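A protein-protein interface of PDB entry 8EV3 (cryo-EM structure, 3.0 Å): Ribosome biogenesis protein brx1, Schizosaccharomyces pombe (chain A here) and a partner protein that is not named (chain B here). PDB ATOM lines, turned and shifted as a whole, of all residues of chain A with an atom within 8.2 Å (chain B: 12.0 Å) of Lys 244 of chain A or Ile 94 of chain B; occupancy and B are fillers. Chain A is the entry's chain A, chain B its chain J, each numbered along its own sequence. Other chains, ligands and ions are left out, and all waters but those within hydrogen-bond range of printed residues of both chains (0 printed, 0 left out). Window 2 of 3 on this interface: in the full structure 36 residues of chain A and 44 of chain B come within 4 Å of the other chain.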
ATOM      1  N   LYS A 123      24.978 -17.126 -27.414  1.00  0.00           N
ATOM      2  CA  LYS A 123      24.030 -17.206 -28.521  1.00  0.00           C
ATOM      3  C   LYS A 123      23.143 -15.969 -28.490  1.00  0.00           C
ATOM      4  O   LYS A 123      22.312 -15.819 -27.589  1.00  0.00           O
ATOM      5  CB  LYS A 123      23.209 -18.490 -28.421  1.00  0.00           C
ATOM      6  CG  LYS A 123      21.989 -18.564 -29.319  1.00  0.00           C
ATOM      7  CD  LYS A 123      21.229 -19.857 -29.054  1.00  0.00           C
ATOM      8  CE  LYS A 123      19.944 -19.930 -29.851  1.00  0.00           C
ATOM      9  NZ  LYS A 123      19.154 -21.150 -29.525  1.00  0.00           N
ATOM     10  N   HIS A 160      27.782 -12.443 -15.980  1.00  0.00           N
ATOM     11  CA  HIS A 160      27.546 -13.015 -17.301  1.00  0.00           C
ATOM     12  C   HIS A 160      27.647 -11.964 -18.399  1.00  0.00           C
ATOM     13  O   HIS A 160      28.138 -12.252 -19.496  1.00  0.00           O
ATOM     14  CB  HIS A 160      26.182 -13.700 -17.337  1.00  0.00           C
ATOM     15  CG  HIS A 160      25.064 -12.865 -16.790  1.00  0.00           C
ATOM     16  ND1 HIS A 160      24.398 -11.918 -17.539  1.00  0.00           N
ATOM     17  CD2 HIS A 160      24.452 -12.884 -15.581  1.00  0.00           C
ATOM     18  CE1 HIS A 160      23.449 -11.364 -16.804  1.00  0.00           C
ATOM     19  NE2 HIS A 160      23.458 -11.935 -15.614  1.00  0.00           N
ATOM     20  N   THR A 228      20.295  -9.674 -28.601  1.00  0.00           N
ATOM     21  CA  THR A 228      19.543 -10.141 -27.444  1.00  0.00           C
ATOM     22  C   THR A 228      20.138 -11.454 -26.950  1.00  0.00           C
ATOM     23  O   THR A 228      20.132 -12.454 -27.675  1.00  0.00           O
ATOM     24  CB  THR A 228      18.068 -10.319 -27.797  1.00  0.00           C
ATOM     25  OG1 THR A 228      17.554  -9.097 -28.338  1.00  0.00           O
ATOM     26  CG2 THR A 228      17.271 -10.693 -26.561  1.00  0.00           C
ATOM     27  N   ILE A 229      20.656 -11.450 -25.719  1.00  0.00           N
ATOM     28  CA  ILE A 229      21.227 -12.665 -25.157  1.00  0.00           C
ATOM     29  C   ILE A 229      20.133 -13.719 -25.023  1.00  0.00           C
ATOM     30  O   ILE A 229      18.957 -13.405 -24.799  1.00  0.00           O
ATOM     31  CB  ILE A 229      21.893 -12.391 -23.798  1.00  0.00           C
ATOM     32  CG1 ILE A 229      22.590 -11.029 -23.799  1.00  0.00           C
ATOM     33  CG2 ILE A 229      22.878 -13.497 -23.449  1.00  0.00           C
ATOM     34  CD1 ILE A 229      23.728 -10.917 -24.783  1.00  0.00           C
ATOM     35  N   ILE A 230      20.517 -14.983 -25.189  1.00  0.00           N
ATOM     36  CA  ILE A 230      19.575 -16.086 -25.048  1.00  0.00           C
ATOM     37  C   ILE A 230      20.096 -17.073 -24.012  1.00  0.00           C
ATOM     38  O   ILE A 230      19.439 -17.328 -22.997  1.00  0.00           O
ATOM     39  CB  ILE A 230      19.317 -16.781 -26.396  1.00  0.00           C
ATOM     40  CG1 ILE A 230      18.786 -15.773 -27.416  1.00  0.00           C
ATOM     41  CG2 ILE A 230      18.342 -17.931 -26.222  1.00  0.00           C
ATOM     42  CD1 ILE A 230      18.554 -16.358 -28.790  1.00  0.00           C
ATOM     43  N   ASN A 231      21.276 -17.633 -24.258  1.00  0.00           N
ATOM     44  CA  ASN A 231      21.872 -18.581 -23.328  1.00  0.00           C
ATOM     45  C   ASN A 231      23.375 -18.617 -23.548  1.00  0.00           C
ATOM     46  O   ASN A 231      23.876 -18.239 -24.609  1.00  0.00           O
ATOM     47  CB  ASN A 231      21.271 -19.981 -23.492  1.00  0.00           C
ATOM     48  CG  ASN A 231      21.307 -20.461 -24.925  1.00  0.00           C
ATOM     49  OD1 ASN A 231      21.294 -19.660 -25.858  1.00  0.00           O
ATOM     50  ND2 ASN A 231      21.356 -21.776 -25.110  1.00  0.00           N
ATOM     51  N   ILE A 232      24.089 -19.075 -22.522  1.00  0.00           N
ATOM     52  CA  ILE A 232      25.535 -19.249 -22.576  1.00  0.00           C
ATOM     53  C   ILE A 232      25.869 -20.635 -22.045  1.00  0.00           C
ATOM     54  O   ILE A 232      25.359 -21.040 -20.994  1.00  0.00           O
ATOM     55  CB  ILE A 232      26.282 -18.167 -21.772  1.00  0.00           C
ATOM     56  CG1 ILE A 232      25.975 -16.775 -22.327  1.00  0.00           C
ATOM     57  CG2 ILE A 232      27.780 -18.422 -21.798  1.00  0.00           C
ATOM     58  CD1 ILE A 232      26.791 -15.672 -21.688  1.00  0.00           C
ATOM     59  N   LEU A 233      26.716 -21.360 -22.769  1.00  0.00           N
ATOM     60  CA  LEU A 233      27.128 -22.702 -22.390  1.00  0.00           C
ATOM     61  C   LEU A 233      28.571 -22.696 -21.903  1.00  0.00           C
ATOM     62  O   LEU A 233      29.332 -21.756 -22.147  1.00  0.00           O
ATOM     63  CB  LEU A 233      26.976 -23.677 -23.562  1.00  0.00           C
ATOM     64  CG  LEU A 233      25.698 -23.582 -24.395  1.00  0.00           C
ATOM     65  CD1 LEU A 233      25.645 -24.710 -25.409  1.00  0.00           C
ATOM     66  CD2 LEU A 233      24.470 -23.610 -23.501  1.00  0.00           C
ATOM     67  N   VAL A 241      24.183 -25.918 -19.909  1.00  0.00           N
ATOM     68  CA  VAL A 241      23.812 -24.509 -19.922  1.00  0.00           C
ATOM     69  C   VAL A 241      24.123 -23.893 -18.565  1.00  0.00           C
ATOM     70  O   VAL A 241      23.870 -24.500 -17.515  1.00  0.00           O
ATOM     71  CB  VAL A 241      22.326 -24.352 -20.276  1.00  0.00           C
ATOM     72  CG1 VAL A 241      22.011 -22.912 -20.646  1.00  0.00           C
ATOM     73  CG2 VAL A 241      21.942 -25.308 -21.396  1.00  0.00           C
ATOM     74  N   ILE A 242      24.686 -22.689 -18.578  1.00  0.00           N
ATOM     75  CA  ILE A 242      24.977 -21.955 -17.354  1.00  0.00           C
ATOM     76  C   ILE A 242      24.237 -20.623 -17.305  1.00  0.00           C
ATOM     77  O   ILE A 242      24.175 -19.985 -16.254  1.00  0.00           O
ATOM     78  CB  ILE A 242      26.503 -21.773 -17.175  1.00  0.00           C
ATOM     79  CG1 ILE A 242      27.166 -21.070 -18.373  1.00  0.00           C
ATOM     80  CG2 ILE A 242      27.172 -23.113 -16.880  1.00  0.00           C
ATOM     81  CD1 ILE A 242      27.045 -19.553 -18.400  1.00  0.00           C
ATOM     82  N   TYR A 243      23.675 -20.185 -18.430  1.00  0.00           N
ATOM     83  CA  TYR A 243      22.962 -18.920 -18.488  1.00  0.00           C
ATOM     84  C   TYR A 243      21.691 -19.145 -19.295  1.00  0.00           C
ATOM     85  O   TYR A 243      21.736 -19.752 -20.367  1.00  0.00           O
ATOM     86  CB  TYR A 243      23.828 -17.838 -19.161  1.00  0.00           C
ATOM     87  CG  TYR A 243      23.284 -16.414 -19.204  1.00  0.00           C
ATOM     88  CD1 TYR A 243      21.990 -16.108 -18.824  1.00  0.00           C
ATOM     89  CD2 TYR A 243      24.122 -15.357 -19.512  1.00  0.00           C
ATOM     90  CE1 TYR A 243      21.525 -14.809 -18.832  1.00  0.00           C
ATOM     91  CE2 TYR A 243      23.657 -14.055 -19.544  1.00  0.00           C
ATOM     92  CZ  TYR A 243      22.361 -13.785 -19.192  1.00  0.00           C
ATOM     93  OH  TYR A 243      21.896 -12.489 -19.204  1.00  0.00           O
ATOM     94  N   LYS A 244      20.562 -18.669 -18.776  1.00  0.00           N
ATOM     95  CA  LYS A 244      19.366 -18.460 -19.585  1.00  0.00           C
ATOM     96  C   LYS A 244      18.913 -17.024 -19.380  1.00  0.00           C
ATOM     97  O   LYS A 244      18.623 -16.619 -18.249  1.00  0.00           O
ATOM     98  CB  LYS A 244      18.246 -19.436 -19.225  1.00  0.00           C
ATOM     99  CG  LYS A 244      17.002 -19.178 -20.040  1.00  0.00           C
ATOM    100  CD  LYS A 244      17.255 -19.565 -21.487  1.00  0.00           C
ATOM    101  CE  LYS A 244      16.294 -18.862 -22.433  1.00  0.00           C
ATOM    102  NZ  LYS A 244      16.532 -17.389 -22.496  1.00  0.00           N
ATOM    103  N   ASN A 245      18.863 -16.253 -20.472  1.00  0.00           N
ATOM    104  CA  ASN A 245      18.613 -14.819 -20.352  1.00  0.00           C
ATOM    105  C   ASN A 245      17.201 -14.539 -19.865  1.00  0.00           C
ATOM    106  O   ASN A 245      16.997 -13.690 -18.988  1.00  0.00           O
ATOM    107  CB  ASN A 245      18.862 -14.123 -21.688  1.00  0.00           C
ATOM    108  CG  ASN A 245      19.113 -12.635 -21.529  1.00  0.00           C
ATOM    109  OD1 ASN A 245      19.050 -11.875 -22.494  1.00  0.00           O
ATOM    110  ND2 ASN A 245      19.418 -12.215 -20.307  1.00  0.00           N
ATOM    111  N   ASP A 246      16.216 -15.234 -20.427  1.00  0.00           N
ATOM    112  CA  ASP A 246      14.800 -15.059 -20.118  1.00  0.00           C
ATOM    113  C   ASP A 246      14.309 -13.649 -20.420  1.00  0.00           C
ATOM    114  O   ASP A 246      13.261 -13.238 -19.906  1.00  0.00           O
ATOM    115  CB  ASP A 246      14.495 -15.422 -18.660  1.00  0.00           C
ATOM    116  CG  ASP A 246      14.664 -16.903 -18.381  1.00  0.00           C
ATOM    117  OD1 ASP A 246      14.134 -17.724 -19.158  1.00  0.00           O
ATOM    118  OD2 ASP A 246      15.336 -17.245 -17.385  1.00  0.00           O
ATOM    119  N   THR A 247      15.043 -12.893 -21.235  1.00  0.00           N
ATOM    120  CA  THR A 247      14.607 -11.561 -21.634  1.00  0.00           C
ATOM    121  C   THR A 247      13.401 -11.681 -22.556  1.00  0.00           C
ATOM    122  O   THR A 247      13.503 -12.254 -23.646  1.00  0.00           O
ATOM    123  CB  THR A 247      15.741 -10.807 -22.324  1.00  0.00           C
ATOM    124  OG1 THR A 247      16.527 -11.722 -23.099  1.00  0.00           O
ATOM    125  CG2 THR A 247      16.630 -10.126 -21.294  1.00  0.00           C
ATOM    126  N   PHE A 248      12.274 -11.111 -22.124  1.00  0.00           N
ATOM    127  CA  PHE A 248      10.960 -11.335 -22.719  1.00  0.00           C
ATOM    128  C   PHE A 248      10.812 -12.768 -23.216  1.00  0.00           C
ATOM    129  O   PHE A 248      10.944 -13.715 -22.434  1.00  0.00           O
ATOM    130  CB  PHE A 248      10.662 -10.328 -23.844  1.00  0.00           C
ATOM    131  CG  PHE A 248      11.848  -9.964 -24.701  1.00  0.00           C
ATOM    132  CD1 PHE A 248      12.703  -8.938 -24.327  1.00  0.00           C
ATOM    133  CD2 PHE A 248      12.079 -10.614 -25.902  1.00  0.00           C
ATOM    134  CE1 PHE A 248      13.782  -8.594 -25.118  1.00  0.00           C
ATOM    135  CE2 PHE A 248      13.157 -10.273 -26.697  1.00  0.00           C
ATOM    136  CZ  PHE A 248      14.009  -9.261 -26.304  1.00  0.00           C
ATOM    137  N   VAL A 249      10.544 -12.943 -24.507  1.00  0.00           N
ATOM    138  CA  VAL A 249      10.234 -14.240 -25.079  1.00  0.00           C
ATOM    139  C   VAL A 249      11.039 -14.429 -26.361  1.00  0.00           C
ATOM    140  O   VAL A 249      11.885 -13.610 -26.715  1.00  0.00           O
ATOM    141  CB  VAL A 249       8.725 -14.403 -25.347  1.00  0.00           C
ATOM    142  CG1 VAL A 249       7.996 -14.768 -24.060  1.00  0.00           C
ATOM    143  CG2 VAL A 249       8.152 -13.130 -25.952  1.00  0.00           C
ATOM    144  N   SER A 250      10.774 -15.541 -27.045  1.00  0.00           N
ATOM    145  CA  SER A 250      11.383 -15.858 -28.329  1.00  0.00           C
ATOM    146  C   SER A 250      10.296 -16.180 -29.345  1.00  0.00           C
ATOM    147  O   SER A 250       9.211 -16.648 -28.988  1.00  0.00           O
ATOM    148  CB  SER A 250      12.354 -17.041 -28.212  1.00  0.00           C
ATOM    149  OG  SER A 250      11.663 -18.241 -27.915  1.00  0.00           O
ATOM    150  N   ILE B  94      20.608 -21.841 -14.948  1.00  0.00           N
ATOM    151  CA  ILE B  94      20.219 -20.563 -15.531  1.00  0.00           C
ATOM    152  C   ILE B  94      20.719 -19.412 -14.667  1.00  0.00           C
ATOM    153  O   ILE B  94      20.499 -19.395 -13.455  1.00  0.00           O
ATOM    154  CB  ILE B  94      18.696 -20.479 -15.718  1.00  0.00           C
ATOM    155  N   ASN B  95      21.389 -18.451 -15.307  1.00  0.00           N
ATOM    156  CA  ASN B  95      21.921 -17.266 -14.631  1.00  0.00           C
ATOM    157  C   ASN B  95      22.857 -17.646 -13.485  1.00  0.00           C
ATOM    158  O   ASN B  95      22.802 -17.068 -12.397  1.00  0.00           O
ATOM    159  CB  ASN B  95      20.793 -16.361 -14.135  1.00  0.00           C
ATOM    160  N   ASN B  96      23.726 -18.626 -13.731  1.00  0.00           N
ATOM    161  CA  ASN B  96      24.711 -19.033 -12.735  1.00  0.00           C
ATOM    162  C   ASN B  96      25.810 -17.984 -12.625  1.00  0.00           C
ATOM    163  O   ASN B  96      26.754 -17.979 -13.422  1.00  0.00           O
ATOM    164  CB  ASN B  96      25.303 -20.398 -13.089  1.00  0.00           C
ATOM    165  N   THR B  97      25.690 -17.093 -11.638  1.00  0.00           N
ATOM    166  CA  THR B  97      26.641 -15.991 -11.509  1.00  0.00           C
ATOM    167  C   THR B  97      28.044 -16.494 -11.194  1.00  0.00           C
ATOM    168  O   THR B  97      29.031 -15.968 -11.722  1.00  0.00           O
ATOM    169  CB  THR B  97      26.170 -15.017 -10.430  1.00  0.00           C
ATOM    170  N   VAL B  98      28.155 -17.504 -10.328  1.00  0.00           N
ATOM    171  CA  VAL B  98      29.468 -18.006  -9.929  1.00  0.00           C
ATOM    172  C   VAL B  98      30.199 -18.596 -11.130  1.00  0.00           C
ATOM    173  O   VAL B  98      31.389 -18.337 -11.343  1.00  0.00           O
ATOM    174  CB  VAL B  98      29.327 -19.035  -8.794  1.00  0.00           C
ATOM    175  N   ALA B  99      29.497 -19.404 -11.927  1.00  0.00           N
ATOM    176  CA  ALA B  99      30.114 -19.984 -13.115  1.00  0.00           C
ATOM    177  C   ALA B  99      30.469 -18.911 -14.137  1.00  0.00           C
ATOM    178  O   ALA B  99      31.538 -18.965 -14.756  1.00  0.00           O
ATOM    179  CB  ALA B  99      29.184 -21.029 -13.731  1.00  0.00           C
ATOM    180  N   LEU B 100      29.584 -17.931 -14.329  1.00  0.00           N
ATOM    181  CA  LEU B 100      29.851 -16.868 -15.294  1.00  0.00           C
ATOM    182  C   LEU B 100      31.046 -16.023 -14.871  1.00  0.00           C
ATOM    183  O   LEU B 100      31.857 -15.618 -15.712  1.00  0.00           O
ATOM    184  CB  LEU B 100      28.609 -15.996 -15.469  1.00  0.00           C
ATOM    185  N   GLU B 101      31.168 -15.741 -13.572  1.00  0.00           N
ATOM    186  CA  GLU B 101      32.289 -14.938 -13.092  1.00  0.00           C
ATOM    187  C   GLU B 101      33.618 -15.636 -13.347  1.00  0.00           C
ATOM    188  O   GLU B 101      34.602 -14.994 -13.734  1.00  0.00           O
ATOM    189  CB  GLU B 101      32.116 -14.634 -11.604  1.00  0.00           C
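N of Asn 95 of chain B sits at hydrogen-bond distance from O of Ile 242 of chain A (3.3 Å). The backbone NH (N) of Asn 96 of chain B sits at hydrogen-bond distance from the backbone carbonyl oxygen (O) of Ile 242 of chain A, at 2.9 Å.
The backbone NH of Ile 242 of chain A is in hydrogen-bond range of the backbone carbonyl oxygen of Ile 232 of chain A, 3.0 Å away. N of Tyr 243 of chain A is in hydrogen-bond range of O of Ile 232 of chain A, 3.2 Å away. The side-chain hydroxyl of Tyr 243 of chain A sits at hydrogen-bond distance from the side-chain amide nitrogen of Asn 245 of chain A (2.7 Å). The side-chain hydroxyl of Tyr 243 of chain A lies close to a ring nitrogen (ND1) of His 160 of chain A, at 3.1 Å. NZ of Lys 244 of chain A is in hydrogen-bond range of O of Ile 230 of chain A (3.0 Å).
Among the printed residues, pairs that only touch across the chains: His 160 of chain A with Leu 100 of chain B (3.7 Å), Ile 242 of chain A with Ile 94 of chain B (3.8 Å), Tyr 243 of chain A with Asn 95 of chain B (3.6 Å), Lys 244 of chain A with Ile 94 of chain B (3.7 Å) and Lys 244 of chain A with Asn 95 of chain B (3.6 Å).
Of the printed residues of chain A, Ile 94 of chain B touches Ile 242 and Lys 244. No residue of chain B comes within 4 Å of Ile 230 of chain A. No residue of chain B comes within 4 Å of Asn 231 of chain A. No residue of chain B comes within 4 Å of Ile 232 of chain A. No residue of chain B comes within 4 Å of Val 241 of chain A. Ile 242 of chain A touches three residues of chain B. No residue of chain B comes within 4 Å of Asp 246 of chain A. Asn 95 of chain B touches three residues of chain A. Printed residues of chain B within 4 Å of His 160 of chain A: Leu 100 (3.7 Å). Printed residues of chain A within 4 Å of Asn 96 of chain B: Ile 242 (2.9 Å). Of the printed residues of chain A, Leu 100 of chain B touches His 160 (3.7 Å). The nearest printed residue of chain A that does not touch Asn 96 of chain B is Tyr 243 of chain A (4.8 Å).
Of the 8 printed residues of chain B, 4 touch a printed residue of chain A. Of the 18 printed residues of chain A, 4 touch a printed residue of chain B. Hydrophobic or aromatic side chains of chain A that line the printed part of chain B: His 160. Among the printed residues, no Asp or Glu carboxylate lies within 4 Å of a Lys or Arg side-chain nitrogen of the other chain.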
